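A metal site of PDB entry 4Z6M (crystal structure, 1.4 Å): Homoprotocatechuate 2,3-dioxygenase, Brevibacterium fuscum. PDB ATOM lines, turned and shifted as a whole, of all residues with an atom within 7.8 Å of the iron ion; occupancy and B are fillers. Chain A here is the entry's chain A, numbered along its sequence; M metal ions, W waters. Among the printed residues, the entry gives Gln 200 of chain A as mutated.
The iron ion is bound by OE1 of Glu 267, water W3, water W1, water W2, NE2 of His 214 and NE2 of His 155.
The iron ion has six donor atoms within binding distance.
OE2 of Glu 267 is in hydrogen-bond range of OH of Tyr 257, 3.3 Å away.
NE2 of His 248 is in hydrogen-bond range of OE2 of Glu 267 (2.9 Å).
N of Asn 157 lies within hydrogen-bond range of O of His 214 (3.0 Å).
A ring nitrogen (ND1) of His 214 is in hydrogen-bond range of a ring nitrogen (ND1) of His 213 (2.8 Å).
OE1 of Gln 200 sits close to NE2 of His 155, at 3.3 Å.
O of His 155 sits at hydrogen-bond distance from N of Ala 216 (2.8 Å).
ND1 of His 155 sits at hydrogen-bond distance from OD2 of Asp 154 (2.7 Å).
The side-chain amide nitrogen (NE2) of Gln 200 lies within hydrogen-bond range of the side-chain hydroxyl (OH) of Tyr 269 (3.2 Å).
Water W1 bridges OE2 of Glu 267 (2.9 Å) and NE2 of Gln 200 (3.0 Å).
Water W3 bridges the side-chain amide oxygen of Gln 200 and the side-chain amide nitrogen of Asn 157.
Merely in contact with the iron ion: Gln 200 (3.98 Å).
Along chain A the residues within 4 Å of the iron ion span positions 155 to 267.
The nearest printed residue that does not touch the iron ion is Tyr 257 (4.2 Å).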
ATOM      1  N   ASP A 154       2.580 -18.397  23.504  1.00  0.00           N
ATOM      2  CA  ASP A 154       2.111 -17.344  22.599  1.00  0.00           C
ATOM      3  C   ASP A 154       3.072 -16.197  22.307  1.00  0.00           C
ATOM      4  O   ASP A 154       3.242 -15.836  21.127  1.00  0.00           O
ATOM      5  CB  ASP A 154       0.793 -16.749  23.057  1.00  0.00           C
ATOM      6  CG  ASP A 154       0.169 -15.900  21.947  1.00  0.00           C
ATOM      7  OD1 ASP A 154      -0.378 -16.467  20.974  1.00  0.00           O
ATOM      8  OD2 ASP A 154       0.296 -14.661  22.019  1.00  0.00           O
ATOM      9  N   HIS A 155       3.718 -15.621  23.322  1.00  0.00           N
ATOM     10  CA  HIS A 155       4.569 -14.482  23.071  1.00  0.00           C
ATOM     11  C   HIS A 155       5.460 -14.150  24.257  1.00  0.00           C
ATOM     12  O   HIS A 155       5.272 -14.655  25.377  1.00  0.00           O
ATOM     13  CB  HIS A 155       3.743 -13.227  22.697  1.00  0.00           C
ATOM     14  CG  HIS A 155       2.819 -12.713  23.777  1.00  0.00           C
ATOM     15  ND1 HIS A 155       1.498 -13.080  23.875  1.00  0.00           N
ATOM     16  CD2 HIS A 155       3.010 -11.776  24.737  1.00  0.00           C
ATOM     17  CE1 HIS A 155       0.927 -12.411  24.864  1.00  0.00           C
ATOM     18  NE2 HIS A 155       1.828 -11.603  25.397  1.00  0.00           N
ATOM     19  N   PHE A 156       6.413 -13.257  23.997  1.00  0.00           N
ATOM     20  CA  PHE A 156       7.186 -12.578  25.010  1.00  0.00           C
ATOM     21  C   PHE A 156       6.786 -11.115  25.062  1.00  0.00           C
ATOM     22  O   PHE A 156       6.222 -10.577  24.102  1.00  0.00           O
ATOM     23  CB  PHE A 156       8.689 -12.625  24.668  1.00  0.00           C
ATOM     24  CG  PHE A 156       9.205 -13.998  24.304  1.00  0.00           C
ATOM     25  CD1 PHE A 156       9.041 -15.097  25.160  1.00  0.00           C
ATOM     26  CD2 PHE A 156       9.866 -14.200  23.098  1.00  0.00           C
ATOM     27  CE1 PHE A 156       9.553 -16.330  24.826  1.00  0.00           C
ATOM     28  CE2 PHE A 156      10.382 -15.442  22.766  1.00  0.00           C
ATOM     29  CZ  PHE A 156      10.209 -16.487  23.628  1.00  0.00           C
ATOM     30  N   ASN A 157       7.135 -10.449  26.146  1.00  0.00           N
ATOM     31  CA  ASN A 157       6.968  -8.994  26.233  1.00  0.00           C
ATOM     32  C   ASN A 157       8.180  -8.416  26.965  1.00  0.00           C
ATOM     33  O   ASN A 157       8.526  -8.894  28.050  1.00  0.00           O
ATOM     34  CB  ASN A 157       5.648  -8.651  26.941  1.00  0.00           C
ATOM     35  CG  ASN A 157       5.340  -7.172  26.924  1.00  0.00           C
ATOM     36  OD1 ASN A 157       6.130  -6.351  27.389  1.00  0.00           O
ATOM     37  ND2 ASN A 157       4.180  -6.817  26.355  1.00  0.00           N
ATOM     38  N   TRP A 192       3.207  -3.849  19.690  1.00  0.00           N
ATOM     39  CA  TRP A 192       3.030  -5.300  19.578  1.00  0.00           C
ATOM     40  C   TRP A 192       3.404  -5.710  18.167  1.00  0.00           C
ATOM     41  O   TRP A 192       3.078  -5.011  17.240  1.00  0.00           O
ATOM     42  CB  TRP A 192       1.553  -5.638  19.839  1.00  0.00           C
ATOM     43  CG  TRP A 192       1.123  -5.563  21.273  1.00  0.00           C
ATOM     44  CD1 TRP A 192       0.875  -6.622  22.071  1.00  0.00           C
ATOM     45  CD2 TRP A 192       0.853  -4.391  22.068  1.00  0.00           C
ATOM     46  NE1 TRP A 192       0.472  -6.205  23.308  1.00  0.00           N
ATOM     47  CE2 TRP A 192       0.464  -4.836  23.331  1.00  0.00           C
ATOM     48  CE3 TRP A 192       0.883  -3.025  21.826  1.00  0.00           C
ATOM     49  CZ2 TRP A 192       0.130  -3.970  24.363  1.00  0.00           C
ATOM     50  CZ3 TRP A 192       0.516  -2.168  22.834  1.00  0.00           C
ATOM     51  CH2 TRP A 192       0.164  -2.649  24.113  1.00  0.00           C
ATOM     52  N   GLN A 200       0.948 -11.074  18.280  1.00  0.00           N
ATOM     53  CA  GLN A 200       2.282 -10.838  18.763  1.00  0.00           C
ATOM     54  C   GLN A 200       3.090 -12.142  18.892  1.00  0.00           C
ATOM     55  O   GLN A 200       2.571 -13.194  19.250  1.00  0.00           O
ATOM     56  CB  GLN A 200       2.236 -10.111  20.103  1.00  0.00           C
ATOM     57  CG  GLN A 200       1.310 -10.807  21.088  1.00  0.00           C
ATOM     58  CD  GLN A 200       1.092 -10.031  22.344  1.00  0.00           C
ATOM     59  OE1 GLN A 200       2.034  -9.438  22.886  1.00  0.00           O
ATOM     60  NE2 GLN A 200      -0.139 -10.018  22.834  1.00  0.00           N
ATOM     61  N   ALA A 203       6.728  -8.128  22.072  1.00  0.00           N
ATOM     62  CA  ALA A 203       6.066  -6.856  22.277  1.00  0.00           C
ATOM     63  C   ALA A 203       7.002  -6.013  23.118  1.00  0.00           C
ATOM     64  O   ALA A 203       7.838  -6.540  23.846  1.00  0.00           O
ATOM     65  CB  ALA A 203       4.717  -7.046  22.970  1.00  0.00           C
ATOM     66  N   THR A 205       7.156  -2.858  25.882  1.00  0.00           N
ATOM     67  CA  THR A 205       6.541  -2.032  26.915  1.00  0.00           C
ATOM     68  C   THR A 205       7.557  -0.984  27.320  1.00  0.00           C
ATOM     69  O   THR A 205       8.685  -1.313  27.702  1.00  0.00           O
ATOM     70  CB  THR A 205       6.139  -2.871  28.144  1.00  0.00           C
ATOM     71  OG1 THR A 205       5.188  -3.879  27.733  1.00  0.00           O
ATOM     72  CG2 THR A 205       5.520  -1.996  29.208  1.00  0.00           C
ATOM     73  N   HIS A 213       9.271  -8.393  30.649  1.00  0.00           N
ATOM     74  CA  HIS A 213       7.994  -8.136  31.279  1.00  0.00           C
ATOM     75  C   HIS A 213       7.218  -9.421  31.574  1.00  0.00           C
ATOM     76  O   HIS A 213       6.826  -9.658  32.714  1.00  0.00           O
ATOM     77  CB  HIS A 213       7.123  -7.171  30.466  1.00  0.00           C
ATOM     78  CG  HIS A 213       6.025  -6.581  31.277  1.00  0.00           C
ATOM     79  ND1 HIS A 213       4.881  -7.281  31.595  1.00  0.00           N
ATOM     80  CD2 HIS A 213       5.923  -5.389  31.903  1.00  0.00           C
ATOM     81  CE1 HIS A 213       4.121  -6.552  32.373  1.00  0.00           C
ATOM     82  NE2 HIS A 213       4.725  -5.391  32.570  1.00  0.00           N
ATOM     83  N   HIS A 214       7.033 -10.265  30.562  1.00  0.00           N
ATOM     84  CA  HIS A 214       6.373 -11.560  30.766  1.00  0.00           C
ATOM     85  C   HIS A 214       6.611 -12.522  29.651  1.00  0.00           C
ATOM     86  O   HIS A 214       7.082 -12.145  28.575  1.00  0.00           O
ATOM     87  CB  HIS A 214       4.859 -11.394  31.004  1.00  0.00           C
ATOM     88  CG  HIS A 214       4.121 -10.670  29.924  1.00  0.00           C
ATOM     89  ND1 HIS A 214       3.896  -9.310  29.955  1.00  0.00           N
ATOM     90  CD2 HIS A 214       3.465 -11.122  28.828  1.00  0.00           C
ATOM     91  CE1 HIS A 214       3.134  -8.970  28.913  1.00  0.00           C
ATOM     92  NE2 HIS A 214       2.891 -10.048  28.204  1.00  0.00           N
ATOM     93  N   VAL A 215       6.275 -13.785  29.936  1.00  0.00           N
ATOM     94  CA  VAL A 215       6.095 -14.826  28.939  1.00  0.00           C
ATOM     95  C   VAL A 215       4.618 -15.175  28.982  1.00  0.00           C
ATOM     96  O   VAL A 215       4.058 -15.310  30.072  1.00  0.00           O
ATOM     97  CB  VAL A 215       6.945 -16.073  29.302  1.00  0.00           C
ATOM     98  CG1 VAL A 215       6.745 -17.172  28.286  1.00  0.00           C
ATOM     99  CG2 VAL A 215       8.409 -15.694  29.426  1.00  0.00           C
ATOM    100  N   ALA A 216       4.006 -15.365  27.814  1.00  0.00           N
ATOM    101  CA  ALA A 216       2.579 -15.676  27.715  1.00  0.00           C
ATOM    102  C   ALA A 216       2.313 -17.034  27.109  1.00  0.00           C
ATOM    103  O   ALA A 216       2.884 -17.377  26.073  1.00  0.00           O
ATOM    104  CB  ALA A 216       1.882 -14.627  26.866  1.00  0.00           C
ATOM    105  N   HIS A 248      -8.380  -7.747  27.102  1.00  0.00           N
ATOM    106  CA  HIS A 248      -7.505  -6.665  26.634  1.00  0.00           C
ATOM    107  C   HIS A 248      -8.250  -5.837  25.582  1.00  0.00           C
ATOM    108  O   HIS A 248      -9.059  -6.371  24.813  1.00  0.00           O
ATOM    109  CB  HIS A 248      -6.285  -7.226  25.961  1.00  0.00           C
ATOM    110  CG  HIS A 248      -5.220  -7.719  26.883  1.00  0.00           C
ATOM    111  ND1 HIS A 248      -4.704  -6.973  27.927  1.00  0.00           N
ATOM    112  CD2 HIS A 248      -4.521  -8.891  26.866  1.00  0.00           C
ATOM    113  CE1 HIS A 248      -3.736  -7.671  28.507  1.00  0.00           C
ATOM    114  NE2 HIS A 248      -3.593  -8.815  27.864  1.00  0.00           N
ATOM    115  N   SER A 251      -5.103  -6.239  21.314  1.00  0.00           N
ATOM    116  CA  SER A 251      -5.120  -7.692  21.053  1.00  0.00           C
ATOM    117  C   SER A 251      -6.481  -8.358  21.148  1.00  0.00           C
ATOM    118  O   SER A 251      -6.652  -9.443  20.568  1.00  0.00           O
ATOM    119  CB  SER A 251      -4.097  -8.481  21.884  1.00  0.00           C
ATOM    120  OG  SER A 251      -4.628  -8.792  23.194  1.00  0.00           O
ATOM    121  N   TYR A 255      -7.288 -12.504  29.301  1.00  0.00           N
ATOM    122  CA  TYR A 255      -5.956 -12.549  29.896  1.00  0.00           C
ATOM    123  C   TYR A 255      -5.965 -12.665  31.413  1.00  0.00           C
ATOM    124  O   TYR A 255      -6.975 -12.376  32.091  1.00  0.00           O
ATOM    125  CB  TYR A 255      -5.186 -11.274  29.511  1.00  0.00           C
ATOM    126  CG  TYR A 255      -5.620 -10.031  30.258  1.00  0.00           C
ATOM    127  CD1 TYR A 255      -5.104  -9.716  31.492  1.00  0.00           C
ATOM    128  CD2 TYR A 255      -6.575  -9.149  29.725  1.00  0.00           C
ATOM    129  CE1 TYR A 255      -5.502  -8.590  32.190  1.00  0.00           C
ATOM    130  CE2 TYR A 255      -6.970  -8.022  30.414  1.00  0.00           C
ATOM    131  CZ  TYR A 255      -6.449  -7.747  31.661  1.00  0.00           C
ATOM    132  OH  TYR A 255      -6.815  -6.599  32.340  1.00  0.00           O
ATOM    133  N   LEU A 256      -4.782 -13.011  31.916  1.00  0.00           N
ATOM    134  CA  LEU A 256      -4.498 -13.079  33.339  1.00  0.00           C
ATOM    135  C   LEU A 256      -3.000 -12.918  33.525  1.00  0.00           C
ATOM    136  O   LEU A 256      -2.253 -13.477  32.728  1.00  0.00           O
ATOM    137  CB  LEU A 256      -4.918 -14.445  33.906  1.00  0.00           C
ATOM    138  CG  LEU A 256      -4.649 -14.709  35.390  1.00  0.00           C
ATOM    139  CD1 LEU A 256      -5.464 -13.782  36.272  1.00  0.00           C
ATOM    140  CD2 LEU A 256      -4.858 -16.163  35.709  1.00  0.00           C
ATOM    141  N   TYR A 257      -2.554 -12.185  34.551  1.00  0.00           N
ATOM    142  CA  TYR A 257      -1.130 -12.162  34.891  1.00  0.00           C
ATOM    143  C   TYR A 257      -0.899 -12.717  36.297  1.00  0.00           C
ATOM    144  O   TYR A 257      -1.557 -12.286  37.252  1.00  0.00           O
ATOM    145  CB  TYR A 257      -0.560 -10.735  34.821  1.00  0.00           C
ATOM    146  CG  TYR A 257      -0.680 -10.108  33.461  1.00  0.00           C
ATOM    147  CD1 TYR A 257       0.267 -10.303  32.462  1.00  0.00           C
ATOM    148  CD2 TYR A 257      -1.798  -9.321  33.154  1.00  0.00           C
ATOM    149  CE1 TYR A 257       0.142  -9.710  31.219  1.00  0.00           C
ATOM    150  CE2 TYR A 257      -1.930  -8.750  31.930  1.00  0.00           C
ATOM    151  CZ  TYR A 257      -0.971  -8.945  30.958  1.00  0.00           C
ATOM    152  OH  TYR A 257      -1.160  -8.351  29.753  1.00  0.00           O
ATOM    153  N   GLU A 267       1.797 -14.452  31.691  1.00  0.00           N
ATOM    154  CA  GLU A 267       0.455 -14.133  31.197  1.00  0.00           C
ATOM    155  C   GLU A 267      -0.180 -15.419  30.684  1.00  0.00           C
ATOM    156  O   GLU A 267       0.476 -16.240  30.015  1.00  0.00           O
ATOM    157  CB  GLU A 267       0.512 -13.104  30.080  1.00  0.00           C
ATOM    158  CG  GLU A 267      -0.833 -12.597  29.637  1.00  0.00           C
ATOM    159  CD  GLU A 267      -0.784 -11.581  28.528  1.00  0.00           C
ATOM    160  OE1 GLU A 267       0.324 -11.296  28.026  1.00  0.00           O
ATOM    161  OE2 GLU A 267      -1.867 -11.091  28.120  1.00  0.00           O
ATOM    162  N   ILE A 268      -1.477 -15.551  30.942  1.00  0.00           N
ATOM    163  CA  ILE A 268      -2.315 -16.553  30.307  1.00  0.00           C
ATOM    164  C   ILE A 268      -3.278 -15.809  29.393  1.00  0.00           C
ATOM    165  O   ILE A 268      -3.765 -14.758  29.761  1.00  0.00           O
ATOM    166  CB  ILE A 268      -3.092 -17.404  31.346  1.00  0.00           C
ATOM    167  CG1 ILE A 268      -2.268 -17.709  32.630  1.00  0.00           C
ATOM    168  CG2 ILE A 268      -3.621 -18.639  30.627  1.00  0.00           C
ATOM    169  CD1 ILE A 268      -1.072 -18.566  32.374  1.00  0.00           C
ATOM    170  N   TYR A 269      -3.503 -16.320  28.186  1.00  0.00           N
ATOM    171  CA  TYR A 269      -3.985 -15.529  27.072  1.00  0.00           C
ATOM    172  C   TYR A 269      -4.849 -16.386  26.164  1.00  0.00           C
ATOM    173  O   TYR A 269      -4.535 -17.570  25.920  1.00  0.00           O
ATOM    174  CB  TYR A 269      -2.752 -15.072  26.306  1.00  0.00           C
ATOM    175  CG  TYR A 269      -2.852 -14.152  25.124  1.00  0.00           C
ATOM    176  CD1 TYR A 269      -2.788 -12.777  25.287  1.00  0.00           C
ATOM    177  CD2 TYR A 269      -2.887 -14.668  23.846  1.00  0.00           C
ATOM    178  CE1 TYR A 269      -2.747 -11.945  24.177  1.00  0.00           C
ATOM    179  CE2 TYR A 269      -2.858 -13.841  22.741  1.00  0.00           C
ATOM    180  CZ  TYR A 269      -2.782 -12.470  22.909  1.00  0.00           C
ATOM    181  OH  TYR A 269      -2.695 -11.620  21.839  1.00  0.00           O
ATOM    182  N   ARG A 293      -6.128  -1.269  27.792  1.00  0.00           N
ATOM    183  CA  ARG A 293      -5.392  -2.397  28.387  1.00  0.00           C
ATOM    184  C   ARG A 293      -6.350  -3.419  29.004  1.00  0.00           C
ATOM    185  O   ARG A 293      -6.190  -4.629  28.815  1.00  0.00           O
ATOM    186  CB  ARG A 293      -4.378  -1.882  29.416  1.00  0.00           C
ATOM    187  CG  ARG A 293      -3.159  -1.276  28.751  1.00  0.00           C
ATOM    188  CD  ARG A 293      -1.960  -1.193  29.669  1.00  0.00           C
ATOM    189  NE  ARG A 293      -0.778  -0.663  28.988  1.00  0.00           N
ATOM    190  CZ  ARG A 293       0.072  -1.373  28.259  1.00  0.00           C
ATOM    191  NH1 ARG A 293      -0.111  -2.668  28.045  1.00  0.00           N
ATOM    192  NH2 ARG A 293       1.143  -0.801  27.760  1.00  0.00           N
ATOM    193  N   TRP A 304       2.351  -3.758  37.530  1.00  0.00           N
ATOM    194  CA  TRP A 304       2.423  -4.106  36.121  1.00  0.00           C
ATOM    195  C   TRP A 304       3.321  -3.140  35.371  1.00  0.00           C
ATOM    196  O   TRP A 304       4.028  -3.530  34.447  1.00  0.00           O
ATOM    197  CB  TRP A 304       0.993  -4.155  35.508  1.00  0.00           C
ATOM    198  CG  TRP A 304       0.902  -5.020  34.296  1.00  0.00           C
ATOM    199  CD1 TRP A 304       0.654  -6.353  34.261  1.00  0.00           C
ATOM    200  CD2 TRP A 304       1.134  -4.634  32.935  1.00  0.00           C
ATOM    201  NE1 TRP A 304       0.692  -6.825  32.981  1.00  0.00           N
ATOM    202  CE2 TRP A 304       0.988  -5.798  32.138  1.00  0.00           C
ATOM    203  CE3 TRP A 304       1.475  -3.429  32.305  1.00  0.00           C
ATOM    204  CZ2 TRP A 304       1.171  -5.783  30.772  1.00  0.00           C
ATOM    205  CZ3 TRP A 304       1.663  -3.418  30.962  1.00  0.00           C
ATOM    206  CH2 TRP A 304       1.513  -4.577  30.196  1.00  0.00           C
HETATM  207 FE    FE M   1       1.222  -9.955  26.751  1.00  0.00          FE
HETATM  208  O   HOH W   1      -0.725  -9.839  25.819  1.00  0.00           O
HETATM  209  O   HOH W   2       0.530  -8.158  27.826  1.00  0.00           O
HETATM  210  O   HOH W   3       2.135  -8.603  25.339  1.00  0.00           O
